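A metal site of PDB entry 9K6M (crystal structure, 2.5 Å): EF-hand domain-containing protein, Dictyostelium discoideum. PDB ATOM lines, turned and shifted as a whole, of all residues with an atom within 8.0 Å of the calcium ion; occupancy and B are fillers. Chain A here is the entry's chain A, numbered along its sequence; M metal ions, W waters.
Of the 14 residues printed, 5 come within 4 Å of the calcium ion. The nearest printed residue that does not touch the calcium ion is Leu 331 (4.2 Å).
OD1 of Asp 330 lies within hydrogen-bond range of N of Phe 294, at 2.5 Å. OD2 of Asp 324 sits at hydrogen-bond distance from N of Gly 329 (3.1 Å). OE1 of Glu 335 lies within hydrogen-bond range of N of Thr 325.
Water W1 lies within hydrogen-bond range of the side-chain amide nitrogen of Asn 328 (2.8 Å), the side-chain carboxylate of Asp 326 (3.1 Å) and the side-chain carboxylate of Asp 330 (3.3 Å).
The calcium ion is bound by OD1 of Asp 326, 2.2 Å away. The calcium ion is bound by O of Asp 330 (2.2 Å). OD1 of Asp 324 is bound to the calcium ion (2.3 Å). OE2 of Glu 335 is bound to the calcium ion (2.5 Å). The calcium ion is bound by the side-chain amide oxygen (OD1) of Asn 328 (2.7 Å). Slightly farther from the calcium ion lies the side-chain carboxylate (OE1) of Glu 335 (3.0 Å). Slightly farther from the calcium ion lies water W1 (3.0 Å).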
ATOM      1  N   PHE A 294     -26.852 -17.035 -26.378  1.00  0.00           N
ATOM      2  CA  PHE A 294     -28.226 -17.470 -26.228  1.00  0.00           C
ATOM      3  C   PHE A 294     -29.078 -16.246 -25.864  1.00  0.00           C
ATOM      4  O   PHE A 294     -29.378 -15.981 -24.695  1.00  0.00           O
ATOM      5  CB  PHE A 294     -28.327 -18.637 -25.236  1.00  0.00           C
ATOM      6  CG  PHE A 294     -29.483 -19.574 -25.486  1.00  0.00           C
ATOM      7  CD1 PHE A 294     -29.433 -20.490 -26.535  1.00  0.00           C
ATOM      8  CD2 PHE A 294     -30.599 -19.566 -24.673  1.00  0.00           C
ATOM      9  CE1 PHE A 294     -30.489 -21.365 -26.736  1.00  0.00           C
ATOM     10  CE2 PHE A 294     -31.657 -20.429 -24.901  1.00  0.00           C
ATOM     11  CZ  PHE A 294     -31.602 -21.328 -25.933  1.00  0.00           C
ATOM     12  N   TYR A 320     -35.725 -13.564 -19.063  1.00  0.00           N
ATOM     13  CA  TYR A 320     -34.446 -12.871 -19.192  1.00  0.00           C
ATOM     14  C   TYR A 320     -34.257 -11.941 -17.992  1.00  0.00           C
ATOM     15  O   TYR A 320     -33.238 -12.010 -17.308  1.00  0.00           O
ATOM     16  CB  TYR A 320     -34.346 -12.205 -20.561  1.00  0.00           C
ATOM     17  CG  TYR A 320     -33.737 -13.184 -21.558  1.00  0.00           C
ATOM     18  CD1 TYR A 320     -34.497 -14.218 -22.099  1.00  0.00           C
ATOM     19  CD2 TYR A 320     -32.382 -13.131 -21.864  1.00  0.00           C
ATOM     20  CE1 TYR A 320     -33.934 -15.149 -22.962  1.00  0.00           C
ATOM     21  CE2 TYR A 320     -31.804 -14.052 -22.728  1.00  0.00           C
ATOM     22  CZ  TYR A 320     -32.585 -15.064 -23.272  1.00  0.00           C
ATOM     23  OH  TYR A 320     -32.015 -15.981 -24.093  1.00  0.00           O
ATOM     24  N   PHE A 323     -33.529 -13.947 -14.774  1.00  0.00           N
ATOM     25  CA  PHE A 323     -32.448 -14.922 -14.677  1.00  0.00           C
ATOM     26  C   PHE A 323     -31.139 -14.436 -15.305  1.00  0.00           C
ATOM     27  O   PHE A 323     -30.086 -14.976 -14.996  1.00  0.00           O
ATOM     28  CB  PHE A 323     -32.857 -16.237 -15.345  1.00  0.00           C
ATOM     29  CG  PHE A 323     -33.877 -17.037 -14.584  1.00  0.00           C
ATOM     30  CD1 PHE A 323     -33.513 -17.718 -13.440  1.00  0.00           C
ATOM     31  CD2 PHE A 323     -35.191 -17.110 -15.033  1.00  0.00           C
ATOM     32  CE1 PHE A 323     -34.464 -18.448 -12.738  1.00  0.00           C
ATOM     33  CE2 PHE A 323     -36.134 -17.852 -14.333  1.00  0.00           C
ATOM     34  CZ  PHE A 323     -35.764 -18.521 -13.185  1.00  0.00           C
ATOM     35  N   ASP A 324     -31.219 -13.438 -16.177  1.00  0.00           N
ATOM     36  CA  ASP A 324     -30.047 -12.914 -16.881  1.00  0.00           C
ATOM     37  C   ASP A 324     -29.333 -11.917 -15.962  1.00  0.00           C
ATOM     38  O   ASP A 324     -29.380 -10.704 -16.205  1.00  0.00           O
ATOM     39  CB  ASP A 324     -30.471 -12.272 -18.212  1.00  0.00           C
ATOM     40  CG  ASP A 324     -29.351 -11.644 -19.023  1.00  0.00           C
ATOM     41  OD1 ASP A 324     -28.155 -12.051 -18.820  1.00  0.00           O
ATOM     42  OD2 ASP A 324     -29.664 -10.736 -19.836  1.00  0.00           O
ATOM     43  N   THR A 325     -28.638 -12.428 -14.935  1.00  0.00           N
ATOM     44  CA  THR A 325     -28.191 -11.598 -13.820  1.00  0.00           C
ATOM     45  C   THR A 325     -26.956 -10.756 -14.139  1.00  0.00           C
ATOM     46  O   THR A 325     -26.555  -9.961 -13.287  1.00  0.00           O
ATOM     47  CB  THR A 325     -27.883 -12.451 -12.571  1.00  0.00           C
ATOM     48  OG1 THR A 325     -26.843 -13.347 -12.929  1.00  0.00           O
ATOM     49  CG2 THR A 325     -29.077 -13.212 -12.038  1.00  0.00           C
ATOM     50  N   ASP A 326     -26.324 -10.939 -15.310  1.00  0.00           N
ATOM     51  CA  ASP A 326     -25.306 -10.005 -15.776  1.00  0.00           C
ATOM     52  C   ASP A 326     -25.900  -9.063 -16.825  1.00  0.00           C
ATOM     53  O   ASP A 326     -25.173  -8.322 -17.479  1.00  0.00           O
ATOM     54  CB  ASP A 326     -24.066 -10.734 -16.317  1.00  0.00           C
ATOM     55  CG  ASP A 326     -24.305 -11.688 -17.473  1.00  0.00           C
ATOM     56  OD1 ASP A 326     -25.458 -12.100 -17.673  1.00  0.00           O
ATOM     57  OD2 ASP A 326     -23.328 -12.007 -18.169  1.00  0.00           O
ATOM     58  N   LYS A 327     -27.219  -9.094 -17.000  1.00  0.00           N
ATOM     59  CA  LYS A 327     -27.923  -8.218 -17.924  1.00  0.00           C
ATOM     60  C   LYS A 327     -27.278  -8.193 -19.319  1.00  0.00           C
ATOM     61  O   LYS A 327     -27.684  -7.376 -20.138  1.00  0.00           O
ATOM     62  CB  LYS A 327     -28.020  -6.815 -17.315  1.00  0.00           C
ATOM     63  N   ASN A 328     -26.359  -9.121 -19.640  1.00  0.00           N
ATOM     64  CA  ASN A 328     -25.547  -9.008 -20.839  1.00  0.00           C
ATOM     65  C   ASN A 328     -26.316  -9.431 -22.102  1.00  0.00           C
ATOM     66  O   ASN A 328     -25.801  -9.243 -23.205  1.00  0.00           O
ATOM     67  CB  ASN A 328     -24.239  -9.803 -20.759  1.00  0.00           C
ATOM     68  CG  ASN A 328     -24.420 -11.288 -20.984  1.00  0.00           C
ATOM     69  OD1 ASN A 328     -25.511 -11.736 -21.336  1.00  0.00           O
ATOM     70  ND2 ASN A 328     -23.364 -12.045 -20.779  1.00  0.00           N
ATOM     71  N   GLY A 329     -27.498 -10.049 -21.952  1.00  0.00           N
ATOM     72  CA  GLY A 329     -28.369 -10.333 -23.077  1.00  0.00           C
ATOM     73  C   GLY A 329     -28.218 -11.753 -23.632  1.00  0.00           C
ATOM     74  O   GLY A 329     -28.946 -12.126 -24.556  1.00  0.00           O
ATOM     75  N   ASP A 330     -27.270 -12.515 -23.064  1.00  0.00           N
ATOM     76  CA  ASP A 330     -27.057 -13.934 -23.357  1.00  0.00           C
ATOM     77  C   ASP A 330     -27.354 -14.731 -22.098  1.00  0.00           C
ATOM     78  O   ASP A 330     -26.680 -14.544 -21.080  1.00  0.00           O
ATOM     79  CB  ASP A 330     -25.622 -14.211 -23.805  1.00  0.00           C
ATOM     80  CG  ASP A 330     -25.119 -15.646 -23.593  1.00  0.00           C
ATOM     81  OD1 ASP A 330     -25.697 -16.592 -24.179  1.00  0.00           O
ATOM     82  OD2 ASP A 330     -24.142 -15.805 -22.839  1.00  0.00           O
ATOM     83  N   LEU A 331     -28.334 -15.640 -22.167  1.00  0.00           N
ATOM     84  CA  LEU A 331     -28.709 -16.463 -21.034  1.00  0.00           C
ATOM     85  C   LEU A 331     -27.805 -17.680 -20.966  1.00  0.00           C
ATOM     86  O   LEU A 331     -27.941 -18.595 -21.774  1.00  0.00           O
ATOM     87  CB  LEU A 331     -30.183 -16.861 -21.166  1.00  0.00           C
ATOM     88  CG  LEU A 331     -30.746 -17.643 -19.982  1.00  0.00           C
ATOM     89  CD1 LEU A 331     -30.762 -16.775 -18.727  1.00  0.00           C
ATOM     90  CD2 LEU A 331     -32.138 -18.142 -20.300  1.00  0.00           C
ATOM     91  N   ALA A 332     -26.878 -17.679 -20.004  1.00  0.00           N
ATOM     92  CA  ALA A 332     -25.878 -18.731 -19.902  1.00  0.00           C
ATOM     93  C   ALA A 332     -26.448 -19.950 -19.186  1.00  0.00           C
ATOM     94  O   ALA A 332     -27.576 -19.926 -18.701  1.00  0.00           O
ATOM     95  CB  ALA A 332     -24.669 -18.192 -19.166  1.00  0.00           C
ATOM     96  N   LYS A 333     -25.616 -20.985 -19.067  1.00  0.00           N
ATOM     97  CA  LYS A 333     -25.977 -22.198 -18.355  1.00  0.00           C
ATOM     98  C   LYS A 333     -25.924 -21.975 -16.834  1.00  0.00           C
ATOM     99  O   LYS A 333     -26.770 -22.492 -16.106  1.00  0.00           O
ATOM    100  CB  LYS A 333     -25.064 -23.350 -18.773  1.00  0.00           C
ATOM    101  CG  LYS A 333     -25.305 -23.871 -20.182  1.00  0.00           C
ATOM    102  CD  LYS A 333     -24.320 -24.943 -20.600  1.00  0.00           C
ATOM    103  CE  LYS A 333     -24.334 -26.157 -19.697  1.00  0.00           C
ATOM    104  NZ  LYS A 333     -23.621 -27.311 -20.286  1.00  0.00           N
ATOM    105  N   GLU A 335     -26.763 -19.430 -15.432  1.00  0.00           N
ATOM    106  CA  GLU A 335     -27.798 -18.449 -15.104  1.00  0.00           C
ATOM    107  C   GLU A 335     -29.217 -19.022 -15.149  1.00  0.00           C
ATOM    108  O   GLU A 335     -30.117 -18.404 -14.585  1.00  0.00           O
ATOM    109  CB  GLU A 335     -27.720 -17.275 -16.080  1.00  0.00           C
ATOM    110  CG  GLU A 335     -26.424 -16.484 -15.982  1.00  0.00           C
ATOM    111  CD  GLU A 335     -26.406 -15.253 -16.867  1.00  0.00           C
ATOM    112  OE1 GLU A 335     -27.296 -14.415 -16.706  1.00  0.00           O
ATOM    113  OE2 GLU A 335     -25.504 -15.135 -17.725  1.00  0.00           O
HETATM  114 CA    CA M   1     -26.296 -13.344 -19.272  1.00  0.00          CA
HETATM  115  O   HOH W   1     -23.666 -14.606 -19.782  1.00  0.00           O
